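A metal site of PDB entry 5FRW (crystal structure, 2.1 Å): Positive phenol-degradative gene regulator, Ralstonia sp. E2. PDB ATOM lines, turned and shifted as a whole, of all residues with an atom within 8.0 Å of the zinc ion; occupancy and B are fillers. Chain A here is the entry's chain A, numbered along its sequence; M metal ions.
SG of Cys 151 sits close to OE1 of Gln 154 (3.6 Å). The backbone carbonyl oxygen (O) of Cys 185 sits at hydrogen-bond distance from the backbone NH (N) of Trp 130 (2.8 Å). The side-chain sulfur of Cys 177 sits close to the backbone NH of Val 150 (3.3 Å). N of Val 150 sits at hydrogen-bond distance from OE1 of Glu 174 (3.5 Å). The backbone NH of Val 178 sits close to the side-chain sulfur of Cys 185 (3.3 Å). The side-chain sulfur of Cys 151 lies close to the backbone NH of Gly 136, at 3.5 Å. The backbone carbonyl oxygen of Cys 177 sits at hydrogen-bond distance from a ring nitrogen (ND1) of His 182 (3.0 Å). The side-chain sulfur (SG) of Cys 177 lies close to the backbone NH (N) of Gly 179, 3.2 Å away.
Within 4 Å of the zinc ion: Cys 151, Glu 174, Cys 177 and Cys 185. The nearest printed residue that does not touch the zinc ion is Val 178 (4.03 Å).
The zinc ion is bound by OE2 of Glu 174, SG of Cys 185, SG of Cys 151 and SG of Cys 177. The zinc ion has four donor atoms within binding distance.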
ATOM      1  N   VAL A 108       4.882 -33.415  -0.838  1.00  0.00           N
ATOM      2  CA  VAL A 108       5.538 -32.448  -1.690  1.00  0.00           C
ATOM      3  C   VAL A 108       6.995 -32.298  -1.262  1.00  0.00           C
ATOM      4  O   VAL A 108       7.327 -32.508  -0.085  1.00  0.00           O
ATOM      5  CB  VAL A 108       4.777 -31.078  -1.632  1.00  0.00           C
ATOM      6  CG1 VAL A 108       4.831 -30.468  -0.235  1.00  0.00           C
ATOM      7  CG2 VAL A 108       5.322 -30.078  -2.651  1.00  0.00           C
ATOM      8  N   TRP A 130       7.562 -25.471  -3.987  1.00  0.00           N
ATOM      9  CA  TRP A 130       6.965 -26.793  -3.909  1.00  0.00           C
ATOM     10  C   TRP A 130       7.235 -27.570  -5.190  1.00  0.00           C
ATOM     11  O   TRP A 130       6.724 -27.209  -6.242  1.00  0.00           O
ATOM     12  CB  TRP A 130       5.460 -26.711  -3.709  1.00  0.00           C
ATOM     13  CG  TRP A 130       5.006 -26.544  -2.282  1.00  0.00           C
ATOM     14  CD1 TRP A 130       5.768 -26.658  -1.156  1.00  0.00           C
ATOM     15  CD2 TRP A 130       3.676 -26.240  -1.844  1.00  0.00           C
ATOM     16  NE1 TRP A 130       4.980 -26.452  -0.033  1.00  0.00           N
ATOM     17  CE2 TRP A 130       3.692 -26.188  -0.442  1.00  0.00           C
ATOM     18  CE3 TRP A 130       2.471 -26.003  -2.508  1.00  0.00           C
ATOM     19  CZ2 TRP A 130       2.549 -25.919   0.307  1.00  0.00           C
ATOM     20  CZ3 TRP A 130       1.327 -25.727  -1.753  1.00  0.00           C
ATOM     21  CH2 TRP A 130       1.384 -25.702  -0.362  1.00  0.00           C
ATOM     22  N   SER A 133       4.320 -31.677  -6.205  1.00  0.00           N
ATOM     23  CA  SER A 133       3.105 -31.698  -5.390  1.00  0.00           C
ATOM     24  C   SER A 133       2.213 -32.845  -5.829  1.00  0.00           C
ATOM     25  O   SER A 133       1.836 -32.907  -6.999  1.00  0.00           O
ATOM     26  CB  SER A 133       2.332 -30.384  -5.479  1.00  0.00           C
ATOM     27  OG  SER A 133       3.144 -29.285  -5.160  1.00  0.00           O
ATOM     28  N   PHE A 134       1.871 -33.735  -4.903  1.00  0.00           N
ATOM     29  CA  PHE A 134       0.953 -34.821  -5.249  1.00  0.00           C
ATOM     30  C   PHE A 134      -0.382 -34.224  -5.639  1.00  0.00           C
ATOM     31  O   PHE A 134      -1.113 -34.774  -6.462  1.00  0.00           O
ATOM     32  CB  PHE A 134       0.761 -35.786  -4.092  1.00  0.00           C
ATOM     33  CG  PHE A 134      -0.458 -35.500  -3.239  1.00  0.00           C
ATOM     34  CD1 PHE A 134      -1.689 -36.041  -3.560  1.00  0.00           C
ATOM     35  CD2 PHE A 134      -0.362 -34.705  -2.123  1.00  0.00           C
ATOM     36  CE1 PHE A 134      -2.806 -35.782  -2.796  1.00  0.00           C
ATOM     37  CE2 PHE A 134      -1.474 -34.432  -1.330  1.00  0.00           C
ATOM     38  CZ  PHE A 134      -2.701 -34.981  -1.671  1.00  0.00           C
ATOM     39  N   GLU A 135      -0.720 -33.101  -5.030  1.00  0.00           N
ATOM     40  CA  GLU A 135      -2.092 -32.640  -5.132  1.00  0.00           C
ATOM     41  C   GLU A 135      -2.314 -32.017  -6.501  1.00  0.00           C
ATOM     42  O   GLU A 135      -3.359 -32.199  -7.140  1.00  0.00           O
ATOM     43  CB  GLU A 135      -2.392 -31.646  -3.998  1.00  0.00           C
ATOM     44  CG  GLU A 135      -3.839 -31.245  -3.913  1.00  0.00           C
ATOM     45  CD  GLU A 135      -4.194 -30.641  -2.544  1.00  0.00           C
ATOM     46  OE1 GLU A 135      -3.268 -30.237  -1.820  1.00  0.00           O
ATOM     47  OE2 GLU A 135      -5.390 -30.575  -2.216  1.00  0.00           O
ATOM     48  N   GLY A 136      -1.299 -31.292  -6.963  1.00  0.00           N
ATOM     49  CA  GLY A 136      -1.329 -30.714  -8.291  1.00  0.00           C
ATOM     50  C   GLY A 136      -1.481 -31.780  -9.359  1.00  0.00           C
ATOM     51  O   GLY A 136      -2.324 -31.667 -10.242  1.00  0.00           O
ATOM     52  N   ASP A 137      -0.677 -32.841  -9.272  1.00  0.00           N
ATOM     53  CA  ASP A 137      -0.724 -33.911 -10.262  1.00  0.00           C
ATOM     54  C   ASP A 137      -2.058 -34.643 -10.229  1.00  0.00           C
ATOM     55  O   ASP A 137      -2.690 -34.837 -11.275  1.00  0.00           O
ATOM     56  CB  ASP A 137       0.406 -34.912 -10.039  1.00  0.00           C
ATOM     57  CG  ASP A 137       1.752 -34.265  -9.832  1.00  0.00           C
ATOM     58  OD1 ASP A 137       1.880 -33.036 -10.074  1.00  0.00           O
ATOM     59  OD2 ASP A 137       2.703 -34.993  -9.467  1.00  0.00           O
ATOM     60  N   ALA A 148      -7.050 -21.791 -11.466  1.00  0.00           N
ATOM     61  CA  ALA A 148      -6.513 -21.257 -10.209  1.00  0.00           C
ATOM     62  C   ALA A 148      -5.801 -22.401  -9.471  1.00  0.00           C
ATOM     63  O   ALA A 148      -6.181 -23.567  -9.637  1.00  0.00           O
ATOM     64  CB  ALA A 148      -7.623 -20.642  -9.341  1.00  0.00           C
ATOM     65  N   PRO A 149      -4.772 -22.081  -8.660  1.00  0.00           N
ATOM     66  CA  PRO A 149      -3.969 -23.087  -7.926  1.00  0.00           C
ATOM     67  C   PRO A 149      -4.832 -24.114  -7.182  1.00  0.00           C
ATOM     68  O   PRO A 149      -5.907 -23.763  -6.704  1.00  0.00           O
ATOM     69  CB  PRO A 149      -3.155 -22.232  -6.949  1.00  0.00           C
ATOM     70  CG  PRO A 149      -2.988 -20.926  -7.679  1.00  0.00           C
ATOM     71  CD  PRO A 149      -4.296 -20.706  -8.398  1.00  0.00           C
ATOM     72  N   VAL A 150      -4.384 -25.359  -7.132  1.00  0.00           N
ATOM     73  CA  VAL A 150      -5.242 -26.446  -6.647  1.00  0.00           C
ATOM     74  C   VAL A 150      -4.678 -27.248  -5.485  1.00  0.00           C
ATOM     75  O   VAL A 150      -5.296 -28.215  -5.068  1.00  0.00           O
ATOM     76  CB  VAL A 150      -5.576 -27.454  -7.784  1.00  0.00           C
ATOM     77  CG1 VAL A 150      -6.327 -26.763  -8.879  1.00  0.00           C
ATOM     78  CG2 VAL A 150      -4.304 -28.079  -8.313  1.00  0.00           C
ATOM     79  N   CYS A 151      -3.506 -26.891  -4.975  1.00  0.00           N
ATOM     80  CA  CYS A 151      -2.932 -27.659  -3.877  1.00  0.00           C
ATOM     81  C   CYS A 151      -3.580 -27.233  -2.545  1.00  0.00           C
ATOM     82  O   CYS A 151      -2.936 -26.636  -1.680  1.00  0.00           O
ATOM     83  CB  CYS A 151      -1.403 -27.499  -3.891  1.00  0.00           C
ATOM     84  SG  CYS A 151      -0.653 -28.218  -5.442  1.00  0.00           S
ATOM     85  N   TRP A 152      -4.857 -27.593  -2.389  1.00  0.00           N
ATOM     86  CA  TRP A 152      -5.716 -27.165  -1.291  1.00  0.00           C
ATOM     87  C   TRP A 152      -5.315 -27.752   0.048  1.00  0.00           C
ATOM     88  O   TRP A 152      -5.124 -27.034   1.037  1.00  0.00           O
ATOM     89  CB  TRP A 152      -7.169 -27.563  -1.570  1.00  0.00           C
ATOM     90  CG  TRP A 152      -7.745 -27.060  -2.869  1.00  0.00           C
ATOM     91  CD1 TRP A 152      -7.437 -25.892  -3.523  1.00  0.00           C
ATOM     92  CD2 TRP A 152      -8.747 -27.712  -3.661  1.00  0.00           C
ATOM     93  NE1 TRP A 152      -8.173 -25.781  -4.672  1.00  0.00           N
ATOM     94  CE2 TRP A 152      -8.983 -26.886  -4.794  1.00  0.00           C
ATOM     95  CE3 TRP A 152      -9.455 -28.912  -3.535  1.00  0.00           C
ATOM     96  CZ2 TRP A 152      -9.906 -27.228  -5.789  1.00  0.00           C
ATOM     97  CZ3 TRP A 152     -10.375 -29.248  -4.537  1.00  0.00           C
ATOM     98  CH2 TRP A 152     -10.585 -28.404  -5.642  1.00  0.00           C
ATOM     99  N   GLN A 154      -2.513 -29.079   0.648  1.00  0.00           N
ATOM    100  CA  GLN A 154      -1.142 -28.684   0.921  1.00  0.00           C
ATOM    101  C   GLN A 154      -1.047 -27.259   1.524  1.00  0.00           C
ATOM    102  O   GLN A 154      -0.200 -27.008   2.402  1.00  0.00           O
ATOM    103  CB  GLN A 154      -0.291 -28.771  -0.352  1.00  0.00           C
ATOM    104  CG  GLN A 154      -0.364 -30.128  -1.010  1.00  0.00           C
ATOM    105  CD  GLN A 154       0.610 -30.287  -2.148  1.00  0.00           C
ATOM    106  OE1 GLN A 154       1.280 -29.326  -2.566  1.00  0.00           O
ATOM    107  NE2 GLN A 154       0.671 -31.496  -2.684  1.00  0.00           N
ATOM    108  N   ILE A 155      -1.912 -26.343   1.070  1.00  0.00           N
ATOM    109  CA  ILE A 155      -1.928 -24.969   1.596  1.00  0.00           C
ATOM    110  C   ILE A 155      -2.514 -24.970   3.011  1.00  0.00           C
ATOM    111  O   ILE A 155      -2.011 -24.278   3.904  1.00  0.00           O
ATOM    112  CB  ILE A 155      -2.763 -24.038   0.705  1.00  0.00           C
ATOM    113  CG1 ILE A 155      -1.919 -23.575  -0.482  1.00  0.00           C
ATOM    114  CG2 ILE A 155      -3.260 -22.816   1.497  1.00  0.00           C
ATOM    115  CD1 ILE A 155      -0.702 -22.725  -0.038  1.00  0.00           C
ATOM    116  N   GLU A 174      -0.945 -19.880  -2.760  1.00  0.00           N
ATOM    117  CA  GLU A 174      -0.116 -20.327  -3.871  1.00  0.00           C
ATOM    118  C   GLU A 174      -0.021 -19.214  -4.904  1.00  0.00           C
ATOM    119  O   GLU A 174      -1.035 -18.778  -5.405  1.00  0.00           O
ATOM    120  CB  GLU A 174      -0.694 -21.564  -4.528  1.00  0.00           C
ATOM    121  CG  GLU A 174      -0.393 -22.872  -3.842  1.00  0.00           C
ATOM    122  CD  GLU A 174      -0.785 -24.063  -4.716  1.00  0.00           C
ATOM    123  OE1 GLU A 174      -2.002 -24.333  -4.840  1.00  0.00           O
ATOM    124  OE2 GLU A 174       0.114 -24.699  -5.293  1.00  0.00           O
ATOM    125  N   LEU A 175       1.191 -18.747  -5.198  1.00  0.00           N
ATOM    126  CA  LEU A 175       1.402 -17.741  -6.248  1.00  0.00           C
ATOM    127  C   LEU A 175       1.647 -18.388  -7.614  1.00  0.00           C
ATOM    128  O   LEU A 175       1.520 -17.746  -8.654  1.00  0.00           O
ATOM    129  CB  LEU A 175       2.560 -16.827  -5.909  1.00  0.00           C
ATOM    130  CG  LEU A 175       2.513 -16.191  -4.510  1.00  0.00           C
ATOM    131  CD1 LEU A 175       3.642 -15.183  -4.378  1.00  0.00           C
ATOM    132  CD2 LEU A 175       1.156 -15.543  -4.251  1.00  0.00           C
ATOM    133  N   GLU A 176       2.044 -19.655  -7.619  1.00  0.00           N
ATOM    134  CA  GLU A 176       2.033 -20.426  -8.854  1.00  0.00           C
ATOM    135  C   GLU A 176       1.829 -21.895  -8.512  1.00  0.00           C
ATOM    136  O   GLU A 176       2.109 -22.305  -7.392  1.00  0.00           O
ATOM    137  CB  GLU A 176       3.316 -20.200  -9.674  1.00  0.00           C
ATOM    138  CG  GLU A 176       4.634 -20.508  -8.993  1.00  0.00           C
ATOM    139  CD  GLU A 176       5.856 -20.260  -9.889  1.00  0.00           C
ATOM    140  OE1 GLU A 176       5.973 -20.910 -10.957  1.00  0.00           O
ATOM    141  OE2 GLU A 176       6.712 -19.409  -9.535  1.00  0.00           O
ATOM    142  N   CYS A 177       1.319 -22.665  -9.454  1.00  0.00           N
ATOM    143  CA  CYS A 177       0.912 -24.030  -9.160  1.00  0.00           C
ATOM    144  C   CYS A 177       0.965 -24.902 -10.411  1.00  0.00           C
ATOM    145  O   CYS A 177       0.540 -24.480 -11.487  1.00  0.00           O
ATOM    146  CB  CYS A 177      -0.487 -24.037  -8.558  1.00  0.00           C
ATOM    147  SG  CYS A 177      -1.263 -25.684  -8.257  1.00  0.00           S
ATOM    148  N   VAL A 178       1.481 -26.112 -10.243  1.00  0.00           N
ATOM    149  CA  VAL A 178       1.570 -27.065 -11.344  1.00  0.00           C
ATOM    150  C   VAL A 178       0.187 -27.410 -11.877  1.00  0.00           C
ATOM    151  O   VAL A 178       0.035 -27.807 -13.029  1.00  0.00           O
ATOM    152  CB  VAL A 178       2.292 -28.363 -10.925  1.00  0.00           C
ATOM    153  CG1 VAL A 178       3.676 -28.053 -10.456  1.00  0.00           C
ATOM    154  CG2 VAL A 178       1.514 -29.084  -9.836  1.00  0.00           C
ATOM    155  N   GLY A 179      -0.821 -27.257 -11.017  1.00  0.00           N
ATOM    156  CA  GLY A 179      -2.173 -27.605 -11.426  1.00  0.00           C
ATOM    157  C   GLY A 179      -2.622 -26.660 -12.521  1.00  0.00           C
ATOM    158  O   GLY A 179      -3.535 -26.966 -13.290  1.00  0.00           O
ATOM    159  N   CYS A 180      -1.967 -25.510 -12.586  1.00  0.00           N
ATOM    160  CA  CYS A 180      -2.256 -24.498 -13.586  1.00  0.00           C
ATOM    161  C   CYS A 180      -1.331 -24.665 -14.779  1.00  0.00           C
ATOM    162  O   CYS A 180      -1.430 -23.927 -15.758  1.00  0.00           O
ATOM    163  CB  CYS A 180      -2.081 -23.104 -12.984  1.00  0.00           C
ATOM    164  SG  CYS A 180      -3.121 -22.779 -11.548  1.00  0.00           S
ATOM    165  N   HIS A 182       2.211 -24.810 -14.399  1.00  0.00           N
ATOM    166  CA  HIS A 182       3.522 -24.222 -14.163  1.00  0.00           C
ATOM    167  C   HIS A 182       4.501 -25.369 -13.949  1.00  0.00           C
ATOM    168  O   HIS A 182       4.069 -26.503 -13.772  1.00  0.00           O
ATOM    169  CB  HIS A 182       3.506 -23.277 -12.942  1.00  0.00           C
ATOM    170  CG  HIS A 182       2.701 -22.039 -13.146  1.00  0.00           C
ATOM    171  ND1 HIS A 182       1.319 -22.024 -13.095  1.00  0.00           N
ATOM    172  CD2 HIS A 182       3.079 -20.770 -13.414  1.00  0.00           C
ATOM    173  CE1 HIS A 182       0.880 -20.788 -13.309  1.00  0.00           C
ATOM    174  NE2 HIS A 182       1.938 -20.016 -13.507  1.00  0.00           N
ATOM    175  N   HIS A 184       6.294 -25.799 -11.345  1.00  0.00           N
ATOM    176  CA  HIS A 184       6.398 -26.078  -9.916  1.00  0.00           C
ATOM    177  C   HIS A 184       5.367 -25.218  -9.199  1.00  0.00           C
ATOM    178  O   HIS A 184       4.701 -24.392  -9.826  1.00  0.00           O
ATOM    179  CB  HIS A 184       7.805 -25.779  -9.419  1.00  0.00           C
ATOM    180  CG  HIS A 184       8.229 -24.366  -9.675  1.00  0.00           C
ATOM    181  ND1 HIS A 184       8.682 -23.933 -10.891  1.00  0.00           N
ATOM    182  CD2 HIS A 184       8.212 -23.267  -8.868  1.00  0.00           C
ATOM    183  CE1 HIS A 184       8.969 -22.642 -10.826  1.00  0.00           C
ATOM    184  NE2 HIS A 184       8.685 -22.213  -9.616  1.00  0.00           N
ATOM    185  N   CYS A 185       5.221 -25.403  -7.887  1.00  0.00           N
ATOM    186  CA  CYS A 185       4.339 -24.554  -7.110  1.00  0.00           C
ATOM    187  C   CYS A 185       5.190 -23.591  -6.273  1.00  0.00           C
ATOM    188  O   CYS A 185       6.348 -23.875  -5.975  1.00  0.00           O
ATOM    189  CB  CYS A 185       3.399 -25.378  -6.210  1.00  0.00           C
ATOM    190  SG  CYS A 185       2.289 -26.557  -7.037  1.00  0.00           S
ATOM    191  N   ARG A 186       4.624 -22.449  -5.903  1.00  0.00           N
ATOM    192  CA  ARG A 186       5.326 -21.525  -5.028  1.00  0.00           C
ATOM    193  C   ARG A 186       4.313 -20.793  -4.156  1.00  0.00           C
ATOM    194  O   ARG A 186       3.237 -20.421  -4.612  1.00  0.00           O
ATOM    195  CB  ARG A 186       6.189 -20.541  -5.830  1.00  0.00           C
ATOM    196  CG  ARG A 186       7.020 -19.597  -5.004  1.00  0.00           C
ATOM    197  CD  ARG A 186       7.881 -18.713  -5.889  1.00  0.00           C
ATOM    198  NE  ARG A 186       7.050 -17.883  -6.761  1.00  0.00           N
ATOM    199  CZ  ARG A 186       6.504 -16.729  -6.387  1.00  0.00           C
ATOM    200  NH1 ARG A 186       6.699 -16.259  -5.161  1.00  0.00           N
ATOM    201  NH2 ARG A 186       5.755 -16.052  -7.247  1.00  0.00           N
ATOM    202  N   ILE A 187       4.657 -20.641  -2.896  1.00  0.00           N
ATOM    203  CA  ILE A 187       3.715 -20.125  -1.917  1.00  0.00           C
ATOM    204  C   ILE A 187       4.308 -19.002  -1.091  1.00  0.00           C
ATOM    205  O   ILE A 187       5.533 -18.861  -1.020  1.00  0.00           O
ATOM    206  CB  ILE A 187       3.246 -21.242  -0.969  1.00  0.00           C
ATOM    207  CG1 ILE A 187       4.364 -21.572   0.035  1.00  0.00           C
ATOM    208  CG2 ILE A 187       2.840 -22.495  -1.780  1.00  0.00           C
ATOM    209  CD1 ILE A 187       4.008 -22.624   1.103  1.00  0.00           C
HETATM  210 ZN    ZN M   1       0.133 -26.335  -6.450  1.00  0.00          ZN
